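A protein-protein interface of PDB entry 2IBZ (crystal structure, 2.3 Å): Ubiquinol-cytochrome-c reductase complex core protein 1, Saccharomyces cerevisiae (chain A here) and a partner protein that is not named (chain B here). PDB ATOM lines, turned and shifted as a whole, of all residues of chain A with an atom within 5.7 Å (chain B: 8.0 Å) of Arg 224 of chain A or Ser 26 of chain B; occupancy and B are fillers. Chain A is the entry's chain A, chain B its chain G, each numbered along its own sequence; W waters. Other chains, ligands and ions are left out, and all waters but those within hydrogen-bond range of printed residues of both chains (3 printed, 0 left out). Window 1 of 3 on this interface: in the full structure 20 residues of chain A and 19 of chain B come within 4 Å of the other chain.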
ATOM      1  N   GLU A 222      25.193  22.239  -0.057  1.00  0.00           N
ATOM      2  CA  GLU A 222      23.889  22.519   0.532  1.00  0.00           C
ATOM      3  C   GLU A 222      22.908  21.372   0.345  1.00  0.00           C
ATOM      4  O   GLU A 222      23.079  20.546  -0.547  1.00  0.00           O
ATOM      5  CB  GLU A 222      23.291  23.766  -0.132  1.00  0.00           C
ATOM      6  CG  GLU A 222      23.078  23.613  -1.660  1.00  0.00           C
ATOM      7  CD  GLU A 222      22.442  24.834  -2.321  1.00  0.00           C
ATOM      8  OE1 GLU A 222      21.834  24.684  -3.400  1.00  0.00           O
ATOM      9  OE2 GLU A 222      22.551  25.944  -1.770  1.00  0.00           O
ATOM     10  N   VAL A 223      21.901  21.316   1.210  1.00  0.00           N
ATOM     11  CA  VAL A 223      20.831  20.328   1.115  1.00  0.00           C
ATOM     12  C   VAL A 223      19.561  21.140   1.372  1.00  0.00           C
ATOM     13  O   VAL A 223      19.467  21.850   2.357  1.00  0.00           O
ATOM     14  CB  VAL A 223      20.978  19.136   2.126  1.00  0.00           C
ATOM     15  CG1 VAL A 223      21.145  19.619   3.567  1.00  0.00           C
ATOM     16  CG2 VAL A 223      19.764  18.212   2.018  1.00  0.00           C
ATOM     17  N   ARG A 224      18.617  21.107   0.442  1.00  0.00           N
ATOM     18  CA  ARG A 224      17.403  21.895   0.605  1.00  0.00           C
ATOM     19  C   ARG A 224      16.205  20.971   0.746  1.00  0.00           C
ATOM     20  O   ARG A 224      15.880  20.220  -0.163  1.00  0.00           O
ATOM     21  CB  ARG A 224      17.280  22.912  -0.557  1.00  0.00           C
ATOM     22  CG  ARG A 224      18.518  23.837  -0.626  1.00  0.00           C
ATOM     23  CD  ARG A 224      18.716  24.626  -1.936  1.00  0.00           C
ATOM     24  NE  ARG A 224      18.109  25.942  -1.824  1.00  0.00           N
ATOM     25  CZ  ARG A 224      18.752  27.108  -1.867  1.00  0.00           C
ATOM     26  NH1 ARG A 224      18.053  28.208  -1.719  1.00  0.00           N
ATOM     27  NH2 ARG A 224      20.055  27.193  -2.095  1.00  0.00           N
ATOM     28  N   LEU A 225      15.610  20.973   1.933  1.00  0.00           N
ATOM     29  CA  LEU A 225      14.465  20.113   2.246  1.00  0.00           C
ATOM     30  C   LEU A 225      13.160  20.896   2.142  1.00  0.00           C
ATOM     31  O   LEU A 225      12.390  20.964   3.093  1.00  0.00           O
ATOM     32  CB  LEU A 225      14.636  19.531   3.664  1.00  0.00           C
ATOM     33  CG  LEU A 225      15.973  18.811   3.915  1.00  0.00           C
ATOM     34  CD1 LEU A 225      16.558  19.198   5.249  1.00  0.00           C
ATOM     35  CD2 LEU A 225      15.798  17.291   3.832  1.00  0.00           C
ATOM     36  N   ARG A 226      12.888  21.450   0.966  1.00  0.00           N
ATOM     37  CA  ARG A 226      11.684  22.250   0.787  1.00  0.00           C
ATOM     38  C   ARG A 226      10.417  21.535   1.188  1.00  0.00           C
ATOM     39  O   ARG A 226      10.235  20.373   0.868  1.00  0.00           O
ATOM     40  CB  ARG A 226      11.536  22.751  -0.653  1.00  0.00           C
ATOM     41  CG  ARG A 226      10.878  24.125  -0.678  1.00  0.00           C
ATOM     42  CD  ARG A 226       9.818  24.315  -1.732  1.00  0.00           C
ATOM     43  NE  ARG A 226      10.326  25.075  -2.861  1.00  0.00           N
ATOM     44  CZ  ARG A 226       9.601  25.884  -3.624  1.00  0.00           C
ATOM     45  NH1 ARG A 226      10.197  26.514  -4.618  1.00  0.00           N
ATOM     46  NH2 ARG A 226       8.308  26.085  -3.402  1.00  0.00           N
ATOM     47  N   ILE A 407      24.957  24.972   3.637  1.00  0.00           N
ATOM     48  CA  ILE A 407      23.594  25.422   3.912  1.00  0.00           C
ATOM     49  C   ILE A 407      22.629  24.245   4.028  1.00  0.00           C
ATOM     50  O   ILE A 407      22.772  23.261   3.325  1.00  0.00           O
ATOM     51  CB  ILE A 407      23.071  26.344   2.735  1.00  0.00           C
ATOM     52  CG1 ILE A 407      24.056  27.472   2.450  1.00  0.00           C
ATOM     53  CG2 ILE A 407      21.697  26.934   3.052  1.00  0.00           C
ATOM     54  CD1 ILE A 407      23.691  28.281   1.245  1.00  0.00           C
ATOM     55  N   ALA A 408      21.612  24.392   4.871  1.00  0.00           N
ATOM     56  CA  ALA A 408      20.584  23.375   5.035  1.00  0.00           C
ATOM     57  C   ALA A 408      19.309  24.103   5.405  1.00  0.00           C
ATOM     58  O   ALA A 408      19.363  25.089   6.130  1.00  0.00           O
ATOM     59  CB  ALA A 408      20.960  22.406   6.143  1.00  0.00           C
ATOM     60  N   GLY A 409      18.164  23.640   4.907  1.00  0.00           N
ATOM     61  CA  GLY A 409      16.923  24.301   5.262  1.00  0.00           C
ATOM     62  C   GLY A 409      15.688  23.468   4.993  1.00  0.00           C
ATOM     63  O   GLY A 409      15.733  22.525   4.217  1.00  0.00           O
ATOM     64  N   ILE A 413      11.204  27.504   1.927  1.00  0.00           N
ATOM     65  CA  ILE A 413      12.475  28.097   1.518  1.00  0.00           C
ATOM     66  C   ILE A 413      12.605  28.470   0.021  1.00  0.00           C
ATOM     67  O   ILE A 413      13.716  28.514  -0.530  1.00  0.00           O
ATOM     68  CB  ILE A 413      13.669  27.208   1.931  1.00  0.00           C
ATOM     69  CG1 ILE A 413      13.473  25.776   1.437  1.00  0.00           C
ATOM     70  CG2 ILE A 413      13.805  27.186   3.442  1.00  0.00           C
ATOM     71  CD1 ILE A 413      14.694  24.891   1.665  1.00  0.00           C
ATOM     72  N   LEU A 416      14.853  31.396  -0.380  1.00  0.00           N
ATOM     73  CA  LEU A 416      16.269  31.298  -0.042  1.00  0.00           C
ATOM     74  C   LEU A 416      16.937  31.204  -1.396  1.00  0.00           C
ATOM     75  O   LEU A 416      16.688  30.273  -2.148  1.00  0.00           O
ATOM     76  CB  LEU A 416      16.551  30.044   0.808  1.00  0.00           C
ATOM     77  CG  LEU A 416      18.013  29.766   1.199  1.00  0.00           C
ATOM     78  CD1 LEU A 416      18.490  30.769   2.237  1.00  0.00           C
ATOM     79  CD2 LEU A 416      18.170  28.350   1.727  1.00  0.00           C
ATOM     80  N   LEU A 417      17.698  32.217  -1.760  1.00  0.00           N
ATOM     81  CA  LEU A 417      18.350  32.228  -3.063  1.00  0.00           C
ATOM     82  C   LEU A 417      19.382  31.119  -3.268  1.00  0.00           C
ATOM     83  O   LEU A 417      19.721  30.386  -2.342  1.00  0.00           O
ATOM     84  CB  LEU A 417      18.969  33.604  -3.310  1.00  0.00           C
ATOM     85  CG  LEU A 417      18.102  34.637  -4.047  1.00  0.00           C
ATOM     86  CD1 LEU A 417      16.622  34.401  -3.820  1.00  0.00           C
ATOM     87  CD2 LEU A 417      18.518  36.047  -3.673  1.00  0.00           C
ATOM     88  N   ASP A 418      19.861  30.995  -4.498  1.00  0.00           N
ATOM     89  CA  ASP A 418      20.856  29.998  -4.868  1.00  0.00           C
ATOM     90  C   ASP A 418      22.161  30.104  -4.082  1.00  0.00           C
ATOM     91  O   ASP A 418      22.498  31.141  -3.524  1.00  0.00           O
ATOM     92  CB  ASP A 418      21.191  30.147  -6.341  1.00  0.00           C
ATOM     93  CG  ASP A 418      21.668  31.527  -6.654  1.00  0.00           C
ATOM     94  OD1 ASP A 418      20.814  32.429  -6.597  1.00  0.00           O
ATOM     95  OD2 ASP A 418      22.887  31.725  -6.873  1.00  0.00           O
ATOM     96  N   TYR A 419      22.937  29.033  -4.151  1.00  0.00           N
ATOM     97  CA  TYR A 419      24.202  28.946  -3.465  1.00  0.00           C
ATOM     98  C   TYR A 419      25.121  30.113  -3.764  1.00  0.00           C
ATOM     99  O   TYR A 419      25.534  30.809  -2.841  1.00  0.00           O
ATOM    100  CB  TYR A 419      24.898  27.624  -3.802  1.00  0.00           C
ATOM    101  CG  TYR A 419      26.133  27.375  -2.962  1.00  0.00           C
ATOM    102  CD1 TYR A 419      26.030  26.773  -1.701  1.00  0.00           C
ATOM    103  CD2 TYR A 419      27.404  27.762  -3.413  1.00  0.00           C
ATOM    104  CE1 TYR A 419      27.157  26.559  -0.911  1.00  0.00           C
ATOM    105  CE2 TYR A 419      28.540  27.562  -2.628  1.00  0.00           C
ATOM    106  CZ  TYR A 419      28.405  26.955  -1.374  1.00  0.00           C
ATOM    107  OH  TYR A 419      29.512  26.755  -0.581  1.00  0.00           O
ATOM    108  N   ILE A 422      24.485  33.429  -2.101  1.00  0.00           N
ATOM    109  CA  ILE A 422      24.807  33.418  -0.681  1.00  0.00           C
ATOM    110  C   ILE A 422      26.324  33.482  -0.551  1.00  0.00           C
ATOM    111  O   ILE A 422      26.850  34.318   0.162  1.00  0.00           O
ATOM    112  CB  ILE A 422      24.319  32.135   0.030  1.00  0.00           C
ATOM    113  CG1 ILE A 422      22.869  31.798  -0.343  1.00  0.00           C
ATOM    114  CG2 ILE A 422      24.413  32.313   1.524  1.00  0.00           C
ATOM    115  CD1 ILE A 422      21.875  32.870  -0.035  1.00  0.00           C
ATOM    116  N   TRP B  13       9.832  35.666  -5.462  1.00  0.00           N
ATOM    117  CA  TRP B  13      10.449  34.809  -4.447  1.00  0.00           C
ATOM    118  C   TRP B  13       9.604  34.691  -3.183  1.00  0.00           C
ATOM    119  O   TRP B  13       9.301  35.703  -2.529  1.00  0.00           O
ATOM    120  CB  TRP B  13      11.833  35.343  -4.098  1.00  0.00           C
ATOM    121  CG  TRP B  13      12.709  35.433  -5.296  1.00  0.00           C
ATOM    122  CD1 TRP B  13      13.115  36.565  -5.925  1.00  0.00           C
ATOM    123  CD2 TRP B  13      13.296  34.339  -6.009  1.00  0.00           C
ATOM    124  NE1 TRP B  13      13.925  36.249  -6.989  1.00  0.00           N
ATOM    125  CE2 TRP B  13      14.058  34.890  -7.061  1.00  0.00           C
ATOM    126  CE3 TRP B  13      13.257  32.943  -5.854  1.00  0.00           C
ATOM    127  CZ2 TRP B  13      14.790  34.092  -7.965  1.00  0.00           C
ATOM    128  CZ3 TRP B  13      13.986  32.145  -6.750  1.00  0.00           C
ATOM    129  CH2 TRP B  13      14.744  32.724  -7.790  1.00  0.00           C
ATOM    130  N   GLY B  23       8.402  16.747  -0.258  1.00  0.00           N
ATOM    131  CA  GLY B  23       9.025  15.491  -0.620  1.00  0.00           C
ATOM    132  C   GLY B  23      10.251  15.551  -1.508  1.00  0.00           C
ATOM    133  O   GLY B  23      10.976  14.560  -1.632  1.00  0.00           O
ATOM    134  N   ILE B  24      10.466  16.683  -2.172  1.00  0.00           N
ATOM    135  CA  ILE B  24      11.625  16.846  -3.052  1.00  0.00           C
ATOM    136  C   ILE B  24      12.768  17.459  -2.240  1.00  0.00           C
ATOM    137  O   ILE B  24      12.578  18.461  -1.559  1.00  0.00           O
ATOM    138  CB  ILE B  24      11.286  17.787  -4.229  1.00  0.00           C
ATOM    139  CG1 ILE B  24      10.054  17.266  -4.976  1.00  0.00           C
ATOM    140  CG2 ILE B  24      12.499  17.946  -5.152  1.00  0.00           C
ATOM    141  CD1 ILE B  24       9.367  18.292  -5.851  1.00  0.00           C
ATOM    142  N   THR B  25      13.944  16.850  -2.319  1.00  0.00           N
ATOM    143  CA  THR B  25      15.120  17.321  -1.603  1.00  0.00           C
ATOM    144  C   THR B  25      16.227  17.526  -2.628  1.00  0.00           C
ATOM    145  O   THR B  25      16.512  16.619  -3.413  1.00  0.00           O
ATOM    146  CB  THR B  25      15.573  16.259  -0.552  1.00  0.00           C
ATOM    147  OG1 THR B  25      14.535  16.095   0.420  1.00  0.00           O
ATOM    148  CG2 THR B  25      16.861  16.663   0.152  1.00  0.00           C
ATOM    149  N   SER B  26      16.853  18.703  -2.635  1.00  0.00           N
ATOM    150  CA  SER B  26      17.915  18.954  -3.604  1.00  0.00           C
ATOM    151  C   SER B  26      19.268  19.072  -2.948  1.00  0.00           C
ATOM    152  O   SER B  26      19.372  19.412  -1.780  1.00  0.00           O
ATOM    153  CB  SER B  26      17.618  20.200  -4.451  1.00  0.00           C
ATOM    154  OG  SER B  26      17.625  21.381  -3.672  1.00  0.00           O
ATOM    155  N   TYR B  27      20.310  18.789  -3.709  1.00  0.00           N
ATOM    156  CA  TYR B  27      21.665  18.859  -3.186  1.00  0.00           C
ATOM    157  C   TYR B  27      22.540  19.531  -4.218  1.00  0.00           C
ATOM    158  O   TYR B  27      22.327  19.352  -5.417  1.00  0.00           O
ATOM    159  CB  TYR B  27      22.228  17.451  -2.944  1.00  0.00           C
ATOM    160  CG  TYR B  27      21.431  16.575  -2.002  1.00  0.00           C
ATOM    161  CD1 TYR B  27      20.315  15.866  -2.452  1.00  0.00           C
ATOM    162  CD2 TYR B  27      21.834  16.400  -0.677  1.00  0.00           C
ATOM    163  CE1 TYR B  27      19.625  15.007  -1.607  1.00  0.00           C
ATOM    164  CE2 TYR B  27      21.154  15.534   0.176  1.00  0.00           C
ATOM    165  CZ  TYR B  27      20.055  14.840  -0.293  1.00  0.00           C
ATOM    166  OH  TYR B  27      19.395  13.960   0.542  1.00  0.00           O
ATOM    167  N   ALA B  28      23.553  20.258  -3.758  1.00  0.00           N
ATOM    168  CA  ALA B  28      24.478  20.919  -4.663  1.00  0.00           C
ATOM    169  C   ALA B  28      25.829  21.101  -3.968  1.00  0.00           C
ATOM    170  O   ALA B  28      25.917  21.057  -2.742  1.00  0.00           O
ATOM    171  CB  ALA B  28      23.909  22.280  -5.133  1.00  0.00           C
HETATM  172  O   HOH W   1      12.067  17.586   1.502  1.00  0.00           O
HETATM  173  O   HOH W   2       9.777  19.600  -1.688  1.00  0.00           O
HETATM  174  O   HOH W   3      25.340  18.315  -1.128  1.00  0.00           O
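The backbone carbonyl oxygen (O) of Val 223 of chain A is in hydrogen-bond range of the backbone NH (N) of Gly 409 of chain A (3.4 Å). The guanidinium group (NH2) of Arg 224 of chain A lies within salt-bridge range of the side-chain carboxylate (OE2) of Glu 222 of chain A, at 2.8 Å. O of Leu 416 of chain A lies within hydrogen-bond range of NH1 of Arg 224 of chain A. The backbone carbonyl oxygen of Leu 417 of chain A sits at hydrogen-bond distance from the guanidinium group of Arg 224 of chain A (2.8 Å). N of Val 223 of chain A sits at hydrogen-bond distance from O of Ile 407 of chain A. The backbone NH (N) of Leu 225 of chain A is in hydrogen-bond range of the backbone carbonyl oxygen (O) of Gly 409 of chain A (2.8 Å).
Among the printed residues, pairs that only touch across the chains: Arg 224 of chain A with Thr 25 of chain B, Val 223 of chain A with Ser 26 of chain B, Glu 222 of chain A with Tyr 27 of chain B, Val 223 of chain A with Tyr 27 of chain B, Val 223 of chain A with Thr 25 of chain B, Leu 225 of chain A with Thr 25 of chain B, Arg 226 of chain A with Ile 24 of chain B, Leu 417 of chain A with Trp 13 of chain B and Arg 224 of chain A with Ile 24 of chain B.
Water W2 lies within hydrogen-bond range of the backbone carbonyl oxygen of Arg 226 of chain A (2.7 Å), the backbone carbonyl oxygen of Ile 24 of chain B (3.0 Å) and the backbone NH of Gly 23 of chain B (3.5 Å). Water W1 lies within hydrogen-bond range of the side-chain hydroxyl of Thr 25 of chain B (3.1 Å), the backbone carbonyl oxygen of Ile 24 of chain B (3.2 Å) and the backbone carbonyl oxygen of Arg 226 of chain A (3.4 Å). Water W3 bridges O of Glu 222 of chain A and O of Ala 28 of chain B.
Printed residues of chain A that touch a printed residue of chain B: Glu 222, Val 223, Arg 224, Leu 225, Arg 226 and Leu 417. Of the 7 printed residues of chain B, 6 touch a printed residue of chain A. Among the printed residues, 11 pairs touch across the chains.
Of the printed residues of chain A, Ala 28 of chain B touches Glu 222. Of the printed residues of chain B, Val 223 of chain A touches Thr 25 (3.8 Å), Ser 26 (3.4 Å) and Tyr 27 (3.5 Å). Ile 422 of chain A touches none of the printed residues of chain B. The nearest residue of chain A that does not touch Ser 26 of chain B is Glu 222 of chain A (4.1 Å).
The backbone NH of Arg 224 of chain A lies within hydrogen-bond range of the backbone carbonyl oxygen of Ser 26 of chain B. The backbone NH of Glu 222 of chain A lies within hydrogen-bond range of the backbone carbonyl oxygen of Ala 28 of chain B (3.0 Å).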
